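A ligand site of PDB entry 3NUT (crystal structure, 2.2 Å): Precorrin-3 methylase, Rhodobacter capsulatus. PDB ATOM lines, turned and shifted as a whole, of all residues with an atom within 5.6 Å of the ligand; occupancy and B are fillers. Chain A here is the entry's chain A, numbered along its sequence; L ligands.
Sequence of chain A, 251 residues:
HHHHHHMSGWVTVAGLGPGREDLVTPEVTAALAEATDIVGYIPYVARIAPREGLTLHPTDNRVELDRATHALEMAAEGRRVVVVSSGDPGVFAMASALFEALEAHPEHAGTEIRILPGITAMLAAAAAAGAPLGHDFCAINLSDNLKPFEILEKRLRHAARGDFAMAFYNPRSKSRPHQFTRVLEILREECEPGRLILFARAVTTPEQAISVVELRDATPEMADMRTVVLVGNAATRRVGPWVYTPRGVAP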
ATOM      1  N   PRO A  18     -24.768   8.596  20.151  1.00  0.00           N
ATOM      2  CA  PRO A  18     -24.836   7.228  19.661  1.00  0.00           C
ATOM      3  C   PRO A  18     -23.884   6.250  20.333  1.00  0.00           C
ATOM      4  O   PRO A  18     -23.866   5.078  19.958  1.00  0.00           O
ATOM      5  CB  PRO A  18     -24.530   7.374  18.172  1.00  0.00           C
ATOM      6  CG  PRO A  18     -23.686   8.615  18.083  1.00  0.00           C
ATOM      7  CD  PRO A  18     -23.968   9.470  19.277  1.00  0.00           C
ATOM      8  N   GLY A  19     -23.105   6.679  21.321  1.00  0.00           N
ATOM      9  CA  GLY A  19     -22.239   5.743  22.035  1.00  0.00           C
ATOM     10  C   GLY A  19     -20.953   6.351  22.524  1.00  0.00           C
ATOM     11  O   GLY A  19     -20.683   6.307  23.732  1.00  0.00           O
ATOM     12  N   SER A  85     -31.836   8.944  27.293  1.00  0.00           N
ATOM     13  CA  SER A  85     -32.031   8.230  26.029  1.00  0.00           C
ATOM     14  C   SER A  85     -30.755   8.222  25.233  1.00  0.00           C
ATOM     15  O   SER A  85     -30.006   9.198  25.256  1.00  0.00           O
ATOM     16  CB  SER A  85     -33.064   8.958  25.186  1.00  0.00           C
ATOM     17  OG  SER A  85     -34.348   8.581  25.620  1.00  0.00           O
ATOM     18  N   SER A  86     -30.549   7.185  24.458  1.00  0.00           N
ATOM     19  CA  SER A  86     -29.442   7.226  23.497  1.00  0.00           C
ATOM     20  C   SER A  86     -29.793   8.278  22.447  1.00  0.00           C
ATOM     21  O   SER A  86     -30.972   8.661  22.314  1.00  0.00           O
ATOM     22  CB  SER A  86     -29.194   5.842  22.861  1.00  0.00           C
ATOM     23  OG  SER A  86     -30.298   5.494  22.049  1.00  0.00           O
ATOM     24  N   GLY A  87     -28.786   8.770  21.732  1.00  0.00           N
ATOM     25  CA  GLY A  87     -29.009   9.696  20.637  1.00  0.00           C
ATOM     26  C   GLY A  87     -29.592  11.006  21.127  1.00  0.00           C
ATOM     27  O   GLY A  87     -29.105  11.570  22.128  1.00  0.00           O
ATOM     28  N   ASP A  88     -30.616  11.482  20.430  1.00  0.00           N
ATOM     29  CA  ASP A  88     -31.357  12.675  20.842  1.00  0.00           C
ATOM     30  C   ASP A  88     -32.650  12.188  21.480  1.00  0.00           C
ATOM     31  O   ASP A  88     -33.205  11.217  21.027  1.00  0.00           O
ATOM     32  CB  ASP A  88     -31.644  13.556  19.616  1.00  0.00           C
ATOM     33  CG  ASP A  88     -32.345  14.840  19.971  1.00  0.00           C
ATOM     34  OD1 ASP A  88     -31.660  15.901  20.049  1.00  0.00           O
ATOM     35  OD2 ASP A  88     -33.584  14.808  20.187  1.00  0.00           O
ATOM     36  N   PRO A  89     -33.118  12.846  22.564  1.00  0.00           N
ATOM     37  CA  PRO A  89     -34.330  12.335  23.266  1.00  0.00           C
ATOM     38  C   PRO A  89     -35.667  12.636  22.578  1.00  0.00           C
ATOM     39  O   PRO A  89     -36.723  12.097  22.982  1.00  0.00           O
ATOM     40  CB  PRO A  89     -34.261  13.004  24.642  1.00  0.00           C
ATOM     41  CG  PRO A  89     -33.494  14.248  24.428  1.00  0.00           C
ATOM     42  CD  PRO A  89     -32.548  14.027  23.251  1.00  0.00           C
ATOM     43  N   VAL A  91     -36.103  11.956  19.427  1.00  0.00           N
ATOM     44  CA  VAL A  91     -36.068  11.125  18.230  1.00  0.00           C
ATOM     45  C   VAL A  91     -36.422   9.677  18.606  1.00  0.00           C
ATOM     46  O   VAL A  91     -35.565   8.902  19.070  1.00  0.00           O
ATOM     47  CB  VAL A  91     -34.717  11.259  17.479  1.00  0.00           C
ATOM     48  CG1 VAL A  91     -34.698  10.376  16.217  1.00  0.00           C
ATOM     49  CG2 VAL A  91     -34.443  12.705  17.085  1.00  0.00           C
ATOM     50  N   PHE A  92     -37.701   9.323  18.440  1.00  0.00           N
ATOM     51  CA  PHE A  92     -38.201   7.971  18.798  1.00  0.00           C
ATOM     52  C   PHE A  92     -37.679   7.557  20.158  1.00  0.00           C
ATOM     53  O   PHE A  92     -37.000   6.536  20.289  1.00  0.00           O
ATOM     54  CB  PHE A  92     -37.802   6.942  17.725  1.00  0.00           C
ATOM     55  CG  PHE A  92     -38.162   7.380  16.334  1.00  0.00           C
ATOM     56  CD1 PHE A  92     -39.491   7.755  16.039  1.00  0.00           C
ATOM     57  CD2 PHE A  92     -37.197   7.432  15.331  1.00  0.00           C
ATOM     58  CE1 PHE A  92     -39.839   8.189  14.768  1.00  0.00           C
ATOM     59  CE2 PHE A  92     -37.531   7.859  14.047  1.00  0.00           C
ATOM     60  CZ  PHE A  92     -38.858   8.248  13.762  1.00  0.00           C
ATOM     61  N   ALA A  93     -37.970   8.383  21.175  1.00  0.00           N
ATOM     62  CA  ALA A  93     -37.327   8.265  22.494  1.00  0.00           C
ATOM     63  C   ALA A  93     -38.174   8.861  23.597  1.00  0.00           C
ATOM     64  O   ALA A  93     -39.379   9.019  23.424  1.00  0.00           O
ATOM     65  CB  ALA A  93     -35.892   8.867  22.469  1.00  0.00           C
ATOM     66  N   ILE A 119     -26.507  13.917  19.718  1.00  0.00           N
ATOM     67  CA  ILE A 119     -26.217  13.483  18.348  1.00  0.00           C
ATOM     68  C   ILE A 119     -27.115  12.302  18.030  1.00  0.00           C
ATOM     69  O   ILE A 119     -27.059  11.303  18.740  1.00  0.00           O
ATOM     70  CB  ILE A 119     -24.713  13.051  18.212  1.00  0.00           C
ATOM     71  CG1 ILE A 119     -23.746  14.215  18.547  1.00  0.00           C
ATOM     72  CG2 ILE A 119     -24.414  12.464  16.842  1.00  0.00           C
ATOM     73  CD1 ILE A 119     -23.920  15.540  17.724  1.00  0.00           C
ATOM     74  N   THR A 120     -27.964  12.377  16.999  1.00  0.00           N
ATOM     75  CA  THR A 120     -28.754  11.197  16.652  1.00  0.00           C
ATOM     76  C   THR A 120     -27.955  10.283  15.752  1.00  0.00           C
ATOM     77  O   THR A 120     -27.220  10.769  14.873  1.00  0.00           O
ATOM     78  CB  THR A 120     -30.013  11.487  15.852  1.00  0.00           C
ATOM     79  OG1 THR A 120     -29.697  12.371  14.774  1.00  0.00           O
ATOM     80  CG2 THR A 120     -31.080  12.075  16.691  1.00  0.00           C
ATOM     81  N   ALA A 121     -28.164   8.976  15.937  1.00  0.00           N
ATOM     82  CA  ALA A 121     -27.586   7.928  15.116  1.00  0.00           C
ATOM     83  C   ALA A 121     -27.555   8.175  13.614  1.00  0.00           C
ATOM     84  O   ALA A 121     -26.537   7.915  12.971  1.00  0.00           O
ATOM     85  CB  ALA A 121     -28.249   6.585  15.442  1.00  0.00           C
ATOM     86  N   MET A 122     -28.625   8.681  13.036  1.00  0.00           N
ATOM     87  CA  MET A 122     -28.637   8.900  11.583  1.00  0.00           C
ATOM     88  C   MET A 122     -27.526   9.849  11.117  1.00  0.00           C
ATOM     89  O   MET A 122     -26.791   9.554  10.163  1.00  0.00           O
ATOM     90  CB  MET A 122     -30.014   9.386  11.088  1.00  0.00           C
ATOM     91  CG  MET A 122     -30.451  10.784  11.541  1.00  0.00           C
ATOM     92  SD  MET A 122     -32.131  11.182  10.941  1.00  0.00           S
ATOM     93  CE  MET A 122     -31.842  11.136   9.175  1.00  0.00           C
ATOM     94  N   PHE A 168     -33.683   4.888   8.445  1.00  0.00           N
ATOM     95  CA  PHE A 168     -34.520   3.924   9.165  1.00  0.00           C
ATOM     96  C   PHE A 168     -34.003   3.635  10.572  1.00  0.00           C
ATOM     97  O   PHE A 168     -32.886   3.153  10.727  1.00  0.00           O
ATOM     98  CB  PHE A 168     -34.645   2.610   8.375  1.00  0.00           C
ATOM     99  CG  PHE A 168     -35.270   2.785   7.013  1.00  0.00           C
ATOM    100  CD1 PHE A 168     -36.348   3.669   6.829  1.00  0.00           C
ATOM    101  CD2 PHE A 168     -34.792   2.065   5.912  1.00  0.00           C
ATOM    102  CE1 PHE A 168     -36.919   3.828   5.575  1.00  0.00           C
ATOM    103  CE2 PHE A 168     -35.371   2.219   4.637  1.00  0.00           C
ATOM    104  CZ  PHE A 168     -36.425   3.115   4.470  1.00  0.00           C
ATOM    105  N   TYR A 169     -34.825   3.932  11.575  1.00  0.00           N
ATOM    106  CA  TYR A 169     -34.533   3.589  12.952  1.00  0.00           C
ATOM    107  C   TYR A 169     -35.269   2.290  13.303  1.00  0.00           C
ATOM    108  O   TYR A 169     -36.441   2.109  12.953  1.00  0.00           O
ATOM    109  CB  TYR A 169     -34.932   4.726  13.905  1.00  0.00           C
ATOM    110  CG  TYR A 169     -33.994   5.944  13.923  1.00  0.00           C
ATOM    111  CD1 TYR A 169     -33.214   6.238  15.048  1.00  0.00           C
ATOM    112  CD2 TYR A 169     -33.892   6.798  12.829  1.00  0.00           C
ATOM    113  CE1 TYR A 169     -32.361   7.345  15.072  1.00  0.00           C
ATOM    114  CE2 TYR A 169     -33.040   7.901  12.840  1.00  0.00           C
ATOM    115  CZ  TYR A 169     -32.276   8.188  13.968  1.00  0.00           C
ATOM    116  OH  TYR A 169     -31.423   9.295  13.961  1.00  0.00           O
ATOM    117  N   ASN A 170     -34.575   1.389  13.991  1.00  0.00           N
ATOM    118  CA  ASN A 170     -35.175   0.132  14.441  1.00  0.00           C
ATOM    119  C   ASN A 170     -35.562  -0.726  13.244  1.00  0.00           C
ATOM    120  O   ASN A 170     -36.740  -0.966  13.027  1.00  0.00           O
ATOM    121  CB  ASN A 170     -36.385   0.416  15.318  1.00  0.00           C
ATOM    122  CG  ASN A 170     -36.061   1.278  16.494  1.00  0.00           C
ATOM    123  OD1 ASN A 170     -35.248   0.917  17.311  1.00  0.00           O
ATOM    124  ND2 ASN A 170     -36.690   2.433  16.583  1.00  0.00           N
ATOM    125  N   PRO A 171     -34.575  -1.162  12.454  1.00  0.00           N
ATOM    126  CA  PRO A 171     -34.951  -1.807  11.197  1.00  0.00           C
ATOM    127  C   PRO A 171     -35.498  -3.228  11.424  1.00  0.00           C
ATOM    128  O   PRO A 171     -36.534  -3.580  10.849  1.00  0.00           O
ATOM    129  CB  PRO A 171     -33.643  -1.797  10.379  1.00  0.00           C
ATOM    130  CG  PRO A 171     -32.580  -1.197  11.271  1.00  0.00           C
ATOM    131  CD  PRO A 171     -33.124  -1.232  12.674  1.00  0.00           C
ATOM    132  N   ALA A 200     -25.385   0.926   8.392  1.00  0.00           N
ATOM    133  CA  ALA A 200     -24.358   1.448   9.291  1.00  0.00           C
ATOM    134  C   ALA A 200     -24.571   0.909  10.694  1.00  0.00           C
ATOM    135  O   ALA A 200     -25.581   1.175  11.357  1.00  0.00           O
ATOM    136  CB  ALA A 200     -24.312   2.972   9.264  1.00  0.00           C
ATOM    137  N   ARG A 201     -23.602   0.113  11.099  1.00  0.00           N
ATOM    138  CA  ARG A 201     -23.751  -0.720  12.256  1.00  0.00           C
ATOM    139  C   ARG A 201     -22.867  -0.213  13.369  1.00  0.00           C
ATOM    140  O   ARG A 201     -21.665   0.009  13.180  1.00  0.00           O
ATOM    141  CB  ARG A 201     -23.375  -2.171  11.862  1.00  0.00           C
ATOM    142  CG  ARG A 201     -23.246  -3.128  13.033  1.00  0.00           C
ATOM    143  CD  ARG A 201     -22.660  -4.496  12.622  1.00  0.00           C
ATOM    144  NE  ARG A 201     -21.895  -5.098  13.735  1.00  0.00           N
ATOM    145  CZ  ARG A 201     -22.455  -5.591  14.840  1.00  0.00           C
ATOM    146  NH1 ARG A 201     -23.788  -5.555  15.015  1.00  0.00           N
ATOM    147  NH2 ARG A 201     -21.683  -6.129  15.773  1.00  0.00           N
ATOM    148  N   ALA A 202     -23.474  -0.026  14.541  1.00  0.00           N
ATOM    149  CA  ALA A 202     -22.731   0.272  15.779  1.00  0.00           C
ATOM    150  C   ALA A 202     -21.872   1.511  15.600  1.00  0.00           C
ATOM    151  O   ALA A 202     -20.685   1.536  15.943  1.00  0.00           O
ATOM    152  CB  ALA A 202     -21.860  -0.929  16.233  1.00  0.00           C
ATOM    153  N   VAL A 203     -22.506   2.552  15.062  1.00  0.00           N
ATOM    154  CA  VAL A 203     -21.795   3.752  14.664  1.00  0.00           C
ATOM    155  C   VAL A 203     -21.206   4.462  15.887  1.00  0.00           C
ATOM    156  O   VAL A 203     -21.876   4.645  16.891  1.00  0.00           O
ATOM    157  CB  VAL A 203     -22.714   4.672  13.846  1.00  0.00           C
ATOM    158  CG1 VAL A 203     -22.015   5.974  13.548  1.00  0.00           C
ATOM    159  CG2 VAL A 203     -23.069   3.981  12.560  1.00  0.00           C
ATOM    160  N   THR A 204     -19.911   4.800  15.773  1.00  0.00           N
ATOM    161  CA  THR A 204     -19.077   5.458  16.799  1.00  0.00           C
ATOM    162  C   THR A 204     -18.562   4.514  17.878  1.00  0.00           C
ATOM    163  O   THR A 204     -17.970   4.944  18.860  1.00  0.00           O
ATOM    164  CB  THR A 204     -19.735   6.690  17.515  1.00  0.00           C
ATOM    165  OG1 THR A 204     -20.624   6.241  18.538  1.00  0.00           O
ATOM    166  CG2 THR A 204     -20.474   7.593  16.536  1.00  0.00           C
ATOM    167  N   THR A 205     -18.830   3.212  17.712  1.00  0.00           N
ATOM    168  CA  THR A 205     -18.342   2.233  18.677  1.00  0.00           C
ATOM    169  C   THR A 205     -17.176   1.533  17.999  1.00  0.00           C
ATOM    170  O   THR A 205     -16.916   1.758  16.800  1.00  0.00           O
ATOM    171  CB  THR A 205     -19.377   1.182  19.078  1.00  0.00           C
ATOM    172  OG1 THR A 205     -19.395   0.159  18.069  1.00  0.00           O
ATOM    173  CG2 THR A 205     -20.773   1.774  19.266  1.00  0.00           C
ATOM    174  N   ASP A 224     -29.342  -5.195  11.590  1.00  0.00           N
ATOM    175  CA  ASP A 224     -29.808  -5.706  12.906  1.00  0.00           C
ATOM    176  C   ASP A 224     -30.256  -4.531  13.759  1.00  0.00           C
ATOM    177  O   ASP A 224     -30.441  -3.437  13.248  1.00  0.00           O
ATOM    178  CB  ASP A 224     -28.762  -6.567  13.623  1.00  0.00           C
ATOM    179  CG  ASP A 224     -27.356  -6.015  13.504  1.00  0.00           C
ATOM    180  OD1 ASP A 224     -27.104  -4.860  13.916  1.00  0.00           O
ATOM    181  OD2 ASP A 224     -26.482  -6.765  13.015  1.00  0.00           O
ATOM    182  N   MET A 225     -30.468  -4.763  15.056  1.00  0.00           N
ATOM    183  CA  MET A 225     -30.917  -3.669  15.951  1.00  0.00           C
ATOM    184  C   MET A 225     -29.817  -2.676  16.332  1.00  0.00           C
ATOM    185  O   MET A 225     -30.090  -1.662  16.946  1.00  0.00           O
ATOM    186  CB  MET A 225     -31.639  -4.211  17.194  1.00  0.00           C
ATOM    187  CG  MET A 225     -33.118  -4.525  16.912  1.00  0.00           C
ATOM    188  SD  MET A 225     -33.868  -3.262  15.817  1.00  0.00           S
ATOM    189  CE  MET A 225     -34.494  -2.125  17.074  1.00  0.00           C
ATOM    190  N   ARG A 226     -28.597  -2.990  15.921  1.00  0.00           N
ATOM    191  CA  ARG A 226     -27.416  -2.158  16.136  1.00  0.00           C
ATOM    192  C   ARG A 226     -27.162  -1.265  14.901  1.00  0.00           C
ATOM    193  O   ARG A 226     -26.042  -0.753  14.697  1.00  0.00           O
ATOM    194  CB  ARG A 226     -26.222  -3.107  16.381  1.00  0.00           C
ATOM    195  CG  ARG A 226     -25.069  -2.567  17.215  1.00  0.00           C
ATOM    196  CD  ARG A 226     -25.297  -2.598  18.735  1.00  0.00           C
ATOM    197  NE  ARG A 226     -24.352  -1.681  19.397  1.00  0.00           N
ATOM    198  CZ  ARG A 226     -24.557  -0.373  19.599  1.00  0.00           C
ATOM    199  NH1 ARG A 226     -25.691   0.232  19.238  1.00  0.00           N
ATOM    200  NH2 ARG A 226     -23.600   0.334  20.191  1.00  0.00           N
ATOM    201  N   THR A 227     -28.190  -1.092  14.077  1.00  0.00           N
ATOM    202  CA  THR A 227     -28.006  -0.588  12.710  1.00  0.00           C
ATOM    203  C   THR A 227     -29.032   0.484  12.384  1.00  0.00           C
ATOM    204  O   THR A 227     -30.187   0.414  12.811  1.00  0.00           O
ATOM    205  CB  THR A 227     -28.100  -1.753  11.687  1.00  0.00           C
ATOM    206  OG1 THR A 227     -27.121  -2.732  12.036  1.00  0.00           O
ATOM    207  CG2 THR A 227     -27.856  -1.322  10.237  1.00  0.00           C
ATOM    208  N   VAL A 228     -28.582   1.494  11.645  1.00  0.00           N
ATOM    209  CA  VAL A 228     -29.456   2.479  11.094  1.00  0.00           C
ATOM    210  C   VAL A 228     -29.228   2.433   9.571  1.00  0.00           C
ATOM    211  O   VAL A 228     -28.084   2.321   9.110  1.00  0.00           O
ATOM    212  CB  VAL A 228     -29.238   3.895  11.740  1.00  0.00           C
ATOM    213  CG1 VAL A 228     -27.843   4.450  11.440  1.00  0.00           C
ATOM    214  CG2 VAL A 228     -30.298   4.890  11.270  1.00  0.00           C
HETATM  215  N1  LIG L   1     -33.120   8.529  20.304  1.00  0.00           N
HETATM  216  C1  LIG L   1     -32.327   7.618  19.410  1.00  0.00           C
HETATM  217  C2  LIG L   1     -33.257   6.694  18.615  1.00  0.00           C
HETATM  218  C3  LIG L   1     -33.843   5.583  19.485  1.00  0.00           C
HETATM  219  S1  LIG L   1     -34.434   4.192  18.558  1.00  0.00           S
HETATM  220  C4  LIG L   1     -31.573   8.513  18.508  1.00  0.00           C
HETATM  221  O1  LIG L   1     -31.918   9.679  18.542  1.00  0.00           O
HETATM  222  O2  LIG L   1     -30.644   8.154  17.754  1.00  0.00           O
HETATM  223  C5  LIG L   1     -33.017   3.106  18.570  1.00  0.00           C
HETATM  224  C6  LIG L   1     -32.519   2.818  17.146  1.00  0.00           C
HETATM  225  O3  LIG L   1     -31.640   3.879  16.720  1.00  0.00           O
HETATM  226  C7  LIG L   1     -31.705   1.532  16.935  1.00  0.00           C
HETATM  227  O4  LIG L   1     -32.495   0.388  16.569  1.00  0.00           O
HETATM  228  C8  LIG L   1     -30.798   1.874  15.775  1.00  0.00           C
HETATM  229  O5  LIG L   1     -31.488   1.782  14.508  1.00  0.00           O
HETATM  230  C9  LIG L   1     -30.520   3.348  16.008  1.00  0.00           C
HETATM  231  N2  LIG L   1     -29.256   3.547  16.759  1.00  0.00           N
HETATM  232  C10 LIG L   1     -29.112   4.028  18.009  1.00  0.00           C
HETATM  233  N3  LIG L   1     -27.789   4.090  18.348  1.00  0.00           N
HETATM  234  C11 LIG L   1     -27.059   3.645  17.304  1.00  0.00           C
HETATM  235  C12 LIG L   1     -25.608   3.453  16.967  1.00  0.00           C
HETATM  236  N4  LIG L   1     -24.618   3.740  17.852  1.00  0.00           N
HETATM  237  N5  LIG L   1     -25.295   2.959  15.744  1.00  0.00           N
HETATM  238  C13 LIG L   1     -26.238   2.656  14.840  1.00  0.00           C
HETATM  239  N6  LIG L   1     -27.567   2.801  15.082  1.00  0.00           N
HETATM  240  C14 LIG L   1     -28.032   3.288  16.263  1.00  0.00           C
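The backbone carbonyl oxygen (O) of Thr 227 is in hydrogen-bond range of an oxygen (O5) of the ligand, at 2.5 Å.
The backbone carbonyl oxygen of Pro 18 lies within hydrogen-bond range of a nitrogen (N4) of the ligand, 2.6 Å away.
N1 of the ligand sits at hydrogen-bond distance from O of Val 91 (2.8 Å).
The backbone NH of Asp 88 sits at hydrogen-bond distance from an oxygen (O1) of the ligand, at 2.9 Å.
The backbone carbonyl oxygen (O) of Asp 88 sits at hydrogen-bond distance from a nitrogen (N1) of the ligand (2.8 Å).
An oxygen (O5) of the ligand is in hydrogen-bond range of the backbone NH (N) of Asn 170 (3.2 Å).
O4 of the ligand sits at hydrogen-bond distance from OD1 of Asn 170, at 2.9 Å.
N5 of the ligand sits at hydrogen-bond distance from N of Val 203, 2.9 Å away.
O of Val 203 is in hydrogen-bond range of N4 of the ligand, at 3.0 Å.
The backbone carbonyl oxygen (O) of Ser 86 lies within hydrogen-bond range of a nitrogen (N1) of the ligand (2.9 Å).
An oxygen (O4) of the ligand is in hydrogen-bond range of the backbone carbonyl oxygen (O) of Met 225, at 3.2 Å.
An oxygen (O2) of the ligand is in hydrogen-bond range of the backbone NH of Ala 121, at 3.2 Å.
The side-chain hydroxyl (OG1) of Thr 227 lies within hydrogen-bond range of the side-chain carboxylate (OD1) of Asp 224 (2.8 Å).
OH of Tyr 169 lies close to N of Met 122 (3.0 Å).
N of Ala 202 is in hydrogen-bond range of O of Arg 226 (2.7 Å).
The side-chain carboxylate (OD1) of Asp 224 lies within hydrogen-bond range of the backbone NH (N) of Arg 226.
The backbone carbonyl oxygen (O) of Ala 202 is in hydrogen-bond range of the side-chain hydroxyl (OG1) of Thr 205 (2.8 Å).
N of Val 228 sits at hydrogen-bond distance from O of Ala 200, 3.0 Å away.
Merely in contact with the ligand: Gly 87 (3.5 Å), Phe 92 (3.4 Å), Ala 93 (3.5 Å), Thr 120 (3.1 Å), Tyr 169 (3.3 Å), Pro 171 (3.9 Å), Ala 200 (3.8 Å), Ala 202 (3.7 Å), Arg 226 (3.4 Å) and Val 228 (3.8 Å).
19 residues have an atom within 4 Å of the ligand: Pro 18, Ser 86, Gly 87, Asp 88, Val 91, Phe 92, Ala 93, Thr 120, Ala 121, Tyr 169, Asn 170, Pro 171, Ala 200, Ala 202, Val 203, Met 225, Arg 226, Thr 227 and Val 228.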
